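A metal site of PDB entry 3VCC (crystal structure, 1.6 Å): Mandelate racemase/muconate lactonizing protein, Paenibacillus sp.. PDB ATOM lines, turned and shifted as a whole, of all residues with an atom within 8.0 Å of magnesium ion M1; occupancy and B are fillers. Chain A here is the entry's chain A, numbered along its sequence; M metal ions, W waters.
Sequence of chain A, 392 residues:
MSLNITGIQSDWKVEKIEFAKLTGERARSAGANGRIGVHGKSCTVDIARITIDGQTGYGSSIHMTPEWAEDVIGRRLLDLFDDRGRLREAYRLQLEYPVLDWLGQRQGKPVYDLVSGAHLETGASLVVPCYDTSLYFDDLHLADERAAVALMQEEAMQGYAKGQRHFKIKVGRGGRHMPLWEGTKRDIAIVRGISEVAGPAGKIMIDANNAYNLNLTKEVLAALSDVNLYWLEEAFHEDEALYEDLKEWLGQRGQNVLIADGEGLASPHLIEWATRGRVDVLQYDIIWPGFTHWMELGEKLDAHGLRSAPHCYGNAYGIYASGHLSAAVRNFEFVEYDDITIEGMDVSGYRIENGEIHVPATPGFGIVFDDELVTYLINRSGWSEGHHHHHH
Merely in contact with magnesium ion M1: Lys 170. Of the 24 residues printed, 4 come within 4 Å of magnesium ion M1.
Water W1 bridges the side-chain amino group (NZ) of Lys 168 (2.7 Å) and the side-chain carboxylate (OE2) of Glu 336 (3.3 Å). Water W3 lies within hydrogen-bond range of the side-chain carboxylate (OE1) of Glu 234, the side-chain carboxylate (OD1) of Asp 207 and the side-chain amide nitrogen (ND2) of Asn 209. Water W2 lies within hydrogen-bond range of OE1 of Glu 263, ND2 of Asn 209 and NZ of Lys 170.
The backbone carbonyl oxygen (O) of Glu 233 is in hydrogen-bond range of the backbone NH (N) of Ala 208, at 3.1 Å. OD2 of Asp 207 sits close to NZ of Lys 168. N of Glu 233 is in hydrogen-bond range of O of Ile 206 (2.8 Å). The side-chain carboxylate of Glu 233 lies within salt-bridge range of the side-chain amino group of Lys 168 (2.9 Å). OD1 of Asp 207 is in hydrogen-bond range of N of Asn 209 (3.0 Å). The side-chain carboxylate of Glu 233 sits at hydrogen-bond distance from the side-chain amide nitrogen of Gln 283 (2.9 Å). The indole nitrogen of Trp 231 is in hydrogen-bond range of the side-chain carboxylate of Glu 233 (3.2 Å). The side-chain carboxylate (OD2) of Asp 207 lies close to the side-chain amino group (NZ) of Lys 170, at 2.8 Å.
The side-chain carboxylate (OE2) of Glu 233 is bound to magnesium ion M1 (2.1 Å). OE2 of Glu 263 binds magnesium ion M1 (2.2 Å). Water W3 is bound to magnesium ion M1, 2.2 Å away. Magnesium ion M1 is bound by water W1, 2.2 Å away. OD2 of Asp 207 binds magnesium ion M1, 2.3 Å away. Water W2 binds magnesium ion M1 (2.3 Å). Magnesium ion M1 has six donor atoms within binding distance.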
ATOM      1  N   ASN A  33     -25.419 -26.887  -9.333  1.00  0.00           N
ATOM      2  CA  ASN A  33     -26.604 -27.225 -10.100  1.00  0.00           C
ATOM      3  C   ASN A  33     -26.987 -28.684  -9.810  1.00  0.00           C
ATOM      4  O   ASN A  33     -26.416 -29.290  -8.880  1.00  0.00           O
ATOM      5  CB  ASN A  33     -26.398 -26.996 -11.605  1.00  0.00           C
ATOM      6  CG  ASN A  33     -25.397 -27.947 -12.219  1.00  0.00           C
ATOM      7  OD1 ASN A  33     -25.018 -28.946 -11.611  1.00  0.00           O
ATOM      8  ND2 ASN A  33     -24.954 -27.644 -13.447  1.00  0.00           N
ATOM      9  N   TYR A 131     -32.156 -14.482 -22.102  1.00  0.00           N
ATOM     10  CA  TYR A 131     -32.631 -14.827 -20.768  1.00  0.00           C
ATOM     11  C   TYR A 131     -31.489 -14.915 -19.767  1.00  0.00           C
ATOM     12  O   TYR A 131     -30.324 -15.158 -20.130  1.00  0.00           O
ATOM     13  CB  TYR A 131     -33.453 -16.122 -20.770  1.00  0.00           C
ATOM     14  CG  TYR A 131     -32.670 -17.395 -21.031  1.00  0.00           C
ATOM     15  CD1 TYR A 131     -31.938 -18.013 -20.019  1.00  0.00           C
ATOM     16  CD2 TYR A 131     -32.676 -17.980 -22.295  1.00  0.00           C
ATOM     17  CE1 TYR A 131     -31.231 -19.203 -20.270  1.00  0.00           C
ATOM     18  CE2 TYR A 131     -31.984 -19.146 -22.553  1.00  0.00           C
ATOM     19  CZ  TYR A 131     -31.268 -19.751 -21.549  1.00  0.00           C
ATOM     20  OH  TYR A 131     -30.584 -20.925 -21.843  1.00  0.00           O
ATOM     21  N   THR A 133     -29.483 -16.698 -17.176  1.00  0.00           N
ATOM     22  CA  THR A 133     -29.186 -18.109 -16.896  1.00  0.00           C
ATOM     23  C   THR A 133     -28.548 -18.330 -15.514  1.00  0.00           C
ATOM     24  O   THR A 133     -28.167 -19.444 -15.165  1.00  0.00           O
ATOM     25  CB  THR A 133     -28.258 -18.699 -18.015  1.00  0.00           C
ATOM     26  OG1 THR A 133     -28.356 -20.134 -18.037  1.00  0.00           O
ATOM     27  CG2 THR A 133     -26.797 -18.278 -17.816  1.00  0.00           C
ATOM     28  N   TYR A 136     -28.629 -20.335 -10.134  1.00  0.00           N
ATOM     29  CA  TYR A 136     -28.111 -21.622  -9.670  1.00  0.00           C
ATOM     30  C   TYR A 136     -28.650 -21.991  -8.277  1.00  0.00           C
ATOM     31  O   TYR A 136     -29.582 -21.348  -7.783  1.00  0.00           O
ATOM     32  CB  TYR A 136     -26.558 -21.596  -9.734  1.00  0.00           C
ATOM     33  CG  TYR A 136     -26.083 -21.886 -11.151  1.00  0.00           C
ATOM     34  CD1 TYR A 136     -26.408 -21.038 -12.204  1.00  0.00           C
ATOM     35  CD2 TYR A 136     -25.389 -23.051 -11.440  1.00  0.00           C
ATOM     36  CE1 TYR A 136     -26.014 -21.332 -13.514  1.00  0.00           C
ATOM     37  CE2 TYR A 136     -25.009 -23.352 -12.746  1.00  0.00           C
ATOM     38  CZ  TYR A 136     -25.312 -22.490 -13.767  1.00  0.00           C
ATOM     39  OH  TYR A 136     -24.923 -22.795 -15.047  1.00  0.00           O
ATOM     40  N   LYS A 168     -34.024 -18.506 -16.519  1.00  0.00           N
ATOM     41  CA  LYS A 168     -33.885 -19.949 -16.427  1.00  0.00           C
ATOM     42  C   LYS A 168     -33.422 -20.355 -15.032  1.00  0.00           C
ATOM     43  O   LYS A 168     -32.364 -19.946 -14.551  1.00  0.00           O
ATOM     44  CB  LYS A 168     -32.939 -20.536 -17.483  1.00  0.00           C
ATOM     45  CG  LYS A 168     -32.984 -22.061 -17.514  1.00  0.00           C
ATOM     46  CD  LYS A 168     -32.380 -22.667 -18.786  1.00  0.00           C
ATOM     47  CE  LYS A 168     -30.868 -22.631 -18.725  1.00  0.00           C
ATOM     48  NZ  LYS A 168     -30.228 -23.027 -20.036  1.00  0.00           N
ATOM     49  N   LYS A 170     -32.337 -23.151 -12.292  1.00  0.00           N
ATOM     50  CA  LYS A 170     -31.825 -24.496 -12.016  1.00  0.00           C
ATOM     51  C   LYS A 170     -32.729 -25.185 -10.999  1.00  0.00           C
ATOM     52  O   LYS A 170     -33.078 -24.606  -9.966  1.00  0.00           O
ATOM     53  CB  LYS A 170     -30.388 -24.450 -11.476  1.00  0.00           C
ATOM     54  CG  LYS A 170     -29.359 -23.879 -12.427  1.00  0.00           C
ATOM     55  CD  LYS A 170     -29.272 -24.723 -13.693  1.00  0.00           C
ATOM     56  CE  LYS A 170     -28.097 -24.214 -14.547  1.00  0.00           C
ATOM     57  NZ  LYS A 170     -27.965 -24.942 -15.838  1.00  0.00           N
ATOM     58  N   ILE A 206     -36.966 -24.004 -16.852  1.00  0.00           N
ATOM     59  CA  ILE A 206     -36.318 -24.745 -15.778  1.00  0.00           C
ATOM     60  C   ILE A 206     -35.357 -25.763 -16.356  1.00  0.00           C
ATOM     61  O   ILE A 206     -35.590 -26.332 -17.425  1.00  0.00           O
ATOM     62  CB  ILE A 206     -37.310 -25.407 -14.777  1.00  0.00           C
ATOM     63  CG1 ILE A 206     -38.181 -26.465 -15.446  1.00  0.00           C
ATOM     64  CG2 ILE A 206     -38.190 -24.349 -14.088  1.00  0.00           C
ATOM     65  CD1 ILE A 206     -39.187 -27.124 -14.462  1.00  0.00           C
ATOM     66  N   ASP A 207     -34.282 -25.994 -15.622  1.00  0.00           N
ATOM     67  CA  ASP A 207     -33.189 -26.828 -16.089  1.00  0.00           C
ATOM     68  C   ASP A 207     -32.780 -27.746 -14.955  1.00  0.00           C
ATOM     69  O   ASP A 207     -32.253 -27.304 -13.931  1.00  0.00           O
ATOM     70  CB  ASP A 207     -32.031 -25.925 -16.549  1.00  0.00           C
ATOM     71  CG  ASP A 207     -30.836 -26.702 -17.070  1.00  0.00           C
ATOM     72  OD1 ASP A 207     -30.817 -27.942 -16.966  1.00  0.00           O
ATOM     73  OD2 ASP A 207     -29.885 -26.047 -17.553  1.00  0.00           O
ATOM     74  N   ALA A 208     -33.068 -29.048 -15.116  1.00  0.00           N
ATOM     75  CA  ALA A 208     -32.802 -30.008 -14.055  1.00  0.00           C
ATOM     76  C   ALA A 208     -31.410 -30.637 -14.098  1.00  0.00           C
ATOM     77  O   ALA A 208     -31.050 -31.389 -13.183  1.00  0.00           O
ATOM     78  CB  ALA A 208     -33.882 -31.107 -14.039  1.00  0.00           C
ATOM     79  N   ASN A 209     -30.621 -30.335 -15.130  1.00  0.00           N
ATOM     80  CA  ASN A 209     -29.329 -30.978 -15.303  1.00  0.00           C
ATOM     81  C   ASN A 209     -29.398 -32.478 -15.040  1.00  0.00           C
ATOM     82  O   ASN A 209     -28.534 -33.054 -14.386  1.00  0.00           O
ATOM     83  CB  ASN A 209     -28.234 -30.325 -14.469  1.00  0.00           C
ATOM     84  CG  ASN A 209     -27.838 -28.973 -15.014  1.00  0.00           C
ATOM     85  OD1 ASN A 209     -28.324 -27.957 -14.535  1.00  0.00           O
ATOM     86  ND2 ASN A 209     -26.991 -28.954 -16.052  1.00  0.00           N
ATOM     87  N   ASN A 210     -30.431 -33.088 -15.618  1.00  0.00           N
ATOM     88  CA  ASN A 210     -30.639 -34.548 -15.602  1.00  0.00           C
ATOM     89  C   ASN A 210     -30.909 -35.174 -14.231  1.00  0.00           C
ATOM     90  O   ASN A 210     -30.882 -36.408 -14.091  1.00  0.00           O
ATOM     91  CB  ASN A 210     -29.482 -35.265 -16.314  1.00  0.00           C
ATOM     92  CG  ASN A 210     -29.469 -34.993 -17.816  1.00  0.00           C
ATOM     93  OD1 ASN A 210     -30.512 -34.715 -18.426  1.00  0.00           O
ATOM     94  ND2 ASN A 210     -28.271 -35.065 -18.405  1.00  0.00           N
ATOM     95  N   TRP A 231     -40.007 -23.567 -21.162  1.00  0.00           N
ATOM     96  CA  TRP A 231     -39.428 -24.873 -21.479  1.00  0.00           C
ATOM     97  C   TRP A 231     -38.865 -25.617 -20.289  1.00  0.00           C
ATOM     98  O   TRP A 231     -38.582 -25.045 -19.231  1.00  0.00           O
ATOM     99  CB  TRP A 231     -38.429 -24.790 -22.658  1.00  0.00           C
ATOM    100  CG  TRP A 231     -36.982 -24.341 -22.389  1.00  0.00           C
ATOM    101  CD1 TRP A 231     -36.149 -24.713 -21.368  1.00  0.00           C
ATOM    102  CD2 TRP A 231     -36.205 -23.470 -23.234  1.00  0.00           C
ATOM    103  NE1 TRP A 231     -34.911 -24.119 -21.518  1.00  0.00           N
ATOM    104  CE2 TRP A 231     -34.925 -23.339 -22.654  1.00  0.00           C
ATOM    105  CE3 TRP A 231     -36.490 -22.772 -24.421  1.00  0.00           C
ATOM    106  CZ2 TRP A 231     -33.923 -22.545 -23.214  1.00  0.00           C
ATOM    107  CZ3 TRP A 231     -35.477 -21.971 -24.977  1.00  0.00           C
ATOM    108  CH2 TRP A 231     -34.214 -21.869 -24.371  1.00  0.00           C
ATOM    109  N   GLU A 233     -35.780 -28.182 -19.525  1.00  0.00           N
ATOM    110  CA  GLU A 233     -34.486 -28.504 -20.093  1.00  0.00           C
ATOM    111  C   GLU A 233     -33.819 -29.617 -19.282  1.00  0.00           C
ATOM    112  O   GLU A 233     -33.732 -29.541 -18.054  1.00  0.00           O
ATOM    113  CB  GLU A 233     -33.598 -27.252 -20.084  1.00  0.00           C
ATOM    114  CG  GLU A 233     -32.131 -27.519 -20.413  1.00  0.00           C
ATOM    115  CD  GLU A 233     -31.350 -26.214 -20.615  1.00  0.00           C
ATOM    116  OE1 GLU A 233     -31.967 -25.152 -20.804  1.00  0.00           O
ATOM    117  OE2 GLU A 233     -30.108 -26.263 -20.585  1.00  0.00           O
ATOM    118  N   GLU A 234     -33.359 -30.653 -19.990  1.00  0.00           N
ATOM    119  CA  GLU A 234     -32.625 -31.753 -19.379  1.00  0.00           C
ATOM    120  C   GLU A 234     -33.255 -32.283 -18.079  1.00  0.00           C
ATOM    121  O   GLU A 234     -32.603 -32.332 -17.030  1.00  0.00           O
ATOM    122  CB  GLU A 234     -31.155 -31.377 -19.143  1.00  0.00           C
ATOM    123  CG  GLU A 234     -30.375 -31.116 -20.452  1.00  0.00           C
ATOM    124  CD  GLU A 234     -28.903 -31.502 -20.363  1.00  0.00           C
ATOM    125  OE1 GLU A 234     -28.153 -30.921 -19.559  1.00  0.00           O
ATOM    126  OE2 GLU A 234     -28.485 -32.385 -21.135  1.00  0.00           O
ATOM    127  N   ALA A 260     -36.543 -29.099 -24.076  1.00  0.00           N
ATOM    128  CA  ALA A 260     -35.253 -28.573 -24.553  1.00  0.00           C
ATOM    129  C   ALA A 260     -34.130 -29.513 -24.122  1.00  0.00           C
ATOM    130  O   ALA A 260     -34.104 -29.969 -22.994  1.00  0.00           O
ATOM    131  CB  ALA A 260     -35.022 -27.176 -23.991  1.00  0.00           C
ATOM    132  N   ASP A 261     -33.200 -29.802 -25.034  1.00  0.00           N
ATOM    133  CA  ASP A 261     -32.096 -30.694 -24.665  1.00  0.00           C
ATOM    134  C   ASP A 261     -30.930 -30.520 -25.652  1.00  0.00           C
ATOM    135  O   ASP A 261     -31.076 -29.799 -26.638  1.00  0.00           O
ATOM    136  CB  ASP A 261     -32.587 -32.137 -24.653  1.00  0.00           C
ATOM    137  CG  ASP A 261     -31.927 -32.971 -23.573  1.00  0.00           C
ATOM    138  OD1 ASP A 261     -30.707 -32.793 -23.390  1.00  0.00           O
ATOM    139  OD2 ASP A 261     -32.618 -33.802 -22.931  1.00  0.00           O
ATOM    140  N   GLY A 262     -29.791 -31.148 -25.369  1.00  0.00           N
ATOM    141  CA  GLY A 262     -28.708 -31.204 -26.347  1.00  0.00           C
ATOM    142  C   GLY A 262     -27.309 -30.779 -25.902  1.00  0.00           C
ATOM    143  O   GLY A 262     -26.343 -30.963 -26.647  1.00  0.00           O
ATOM    144  N   GLU A 263     -27.173 -30.201 -24.712  1.00  0.00           N
ATOM    145  CA  GLU A 263     -25.847 -29.773 -24.277  1.00  0.00           C
ATOM    146  C   GLU A 263     -24.992 -30.982 -23.863  1.00  0.00           C
ATOM    147  O   GLU A 263     -25.496 -32.087 -23.694  1.00  0.00           O
ATOM    148  CB  GLU A 263     -25.923 -28.760 -23.138  1.00  0.00           C
ATOM    149  CG  GLU A 263     -26.312 -29.402 -21.831  1.00  0.00           C
ATOM    150  CD  GLU A 263     -26.469 -28.372 -20.728  1.00  0.00           C
ATOM    151  OE1 GLU A 263     -25.650 -28.330 -19.792  1.00  0.00           O
ATOM    152  OE2 GLU A 263     -27.413 -27.585 -20.851  1.00  0.00           O
ATOM    153  N   GLY A 264     -23.684 -30.756 -23.708  1.00  0.00           N
ATOM    154  CA  GLY A 264     -22.787 -31.777 -23.178  1.00  0.00           C
ATOM    155  C   GLY A 264     -22.628 -32.971 -24.105  1.00  0.00           C
ATOM    156  O   GLY A 264     -22.644 -32.835 -25.324  1.00  0.00           O
ATOM    157  N   GLN A 283     -29.909 -27.605 -28.030  1.00  0.00           N
ATOM    158  CA  GLN A 283     -29.059 -26.757 -27.206  1.00  0.00           C
ATOM    159  C   GLN A 283     -27.574 -27.065 -27.264  1.00  0.00           C
ATOM    160  O   GLN A 283     -26.841 -26.868 -26.291  1.00  0.00           O
ATOM    161  CB  GLN A 283     -29.552 -26.761 -25.752  1.00  0.00           C
ATOM    162  CG  GLN A 283     -30.991 -26.303 -25.630  1.00  0.00           C
ATOM    163  CD  GLN A 283     -31.451 -26.211 -24.184  1.00  0.00           C
ATOM    164  OE1 GLN A 283     -31.530 -27.210 -23.492  1.00  0.00           O
ATOM    165  NE2 GLN A 283     -31.719 -24.997 -23.731  1.00  0.00           N
ATOM    166  N   HIS A 311     -26.446 -23.477 -26.315  1.00  0.00           N
ATOM    167  CA  HIS A 311     -25.968 -23.397 -24.939  1.00  0.00           C
ATOM    168  C   HIS A 311     -24.786 -22.453 -24.854  1.00  0.00           C
ATOM    169  O   HIS A 311     -23.893 -22.465 -25.708  1.00  0.00           O
ATOM    170  CB  HIS A 311     -25.529 -24.783 -24.465  1.00  0.00           C
ATOM    171  CG  HIS A 311     -24.787 -24.782 -23.170  1.00  0.00           C
ATOM    172  ND1 HIS A 311     -23.435 -24.519 -23.072  1.00  0.00           N
ATOM    173  CD2 HIS A 311     -25.215 -25.039 -21.904  1.00  0.00           C
ATOM    174  CE1 HIS A 311     -23.062 -24.596 -21.806  1.00  0.00           C
ATOM    175  NE2 HIS A 311     -24.119 -24.923 -21.087  1.00  0.00           N
ATOM    176  N   CYS A 312     -24.767 -21.632 -23.815  1.00  0.00           N
ATOM    177  CA  CYS A 312     -23.593 -20.833 -23.525  1.00  0.00           C
ATOM    178  C   CYS A 312     -23.499 -20.645 -22.034  1.00  0.00           C
ATOM    179  O   CYS A 312     -24.352 -20.003 -21.418  1.00  0.00           O
ATOM    180  CB  CYS A 312     -23.656 -19.466 -24.206  1.00  0.00           C
ATOM    181  SG  CYS A 312     -22.141 -18.520 -23.943  1.00  0.00           S
ATOM    182  N   TYR A 313     -22.452 -21.216 -21.464  1.00  0.00           N
ATOM    183  CA  TYR A 313     -22.138 -21.038 -20.051  1.00  0.00           C
ATOM    184  C   TYR A 313     -20.702 -21.487 -19.857  1.00  0.00           C
ATOM    185  O   TYR A 313     -20.320 -22.532 -20.393  1.00  0.00           O
ATOM    186  CB  TYR A 313     -23.060 -21.828 -19.139  1.00  0.00           C
ATOM    187  CG  TYR A 313     -22.979 -21.339 -17.710  1.00  0.00           C
ATOM    188  CD1 TYR A 313     -23.728 -20.243 -17.302  1.00  0.00           C
ATOM    189  CD2 TYR A 313     -22.114 -21.923 -16.783  1.00  0.00           C
ATOM    190  CE1 TYR A 313     -23.657 -19.775 -15.986  1.00  0.00           C
ATOM    191  CE2 TYR A 313     -22.024 -21.446 -15.481  1.00  0.00           C
ATOM    192  CZ  TYR A 313     -22.799 -20.366 -15.095  1.00  0.00           C
ATOM    193  OH  TYR A 313     -22.741 -19.884 -13.796  1.00  0.00           O
ATOM    194  N   GLU A 336     -28.405 -17.061 -24.309  1.00  0.00           N
ATOM    195  CA  GLU A 336     -28.275 -17.452 -22.908  1.00  0.00           C
ATOM    196  C   GLU A 336     -27.276 -16.496 -22.248  1.00  0.00           C
ATOM    197  O   GLU A 336     -26.095 -16.490 -22.584  1.00  0.00           O
ATOM    198  CB  GLU A 336     -27.796 -18.901 -22.809  1.00  0.00           C
ATOM    199  CG  GLU A 336     -27.595 -19.416 -21.398  1.00  0.00           C
ATOM    200  CD  GLU A 336     -27.464 -20.926 -21.342  1.00  0.00           C
ATOM    201  OE1 GLU A 336     -27.254 -21.572 -22.392  1.00  0.00           O
ATOM    202  OE2 GLU A 336     -27.594 -21.467 -20.227  1.00  0.00           O
HETATM  203 MG    MG M   1     -28.591 -26.751 -19.254  1.00  0.00          MG
HETATM  204 MG    MG M   2     -29.242 -33.984 -22.361  1.00  0.00          MG
HETATM  205  O   HOH W   1     -28.046 -24.625 -19.586  1.00  0.00           O
HETATM  206  O   HOH W   2     -26.630 -26.894 -17.970  1.00  0.00           O
HETATM  207  O   HOH W   3     -28.922 -28.824 -18.577  1.00  0.00           O
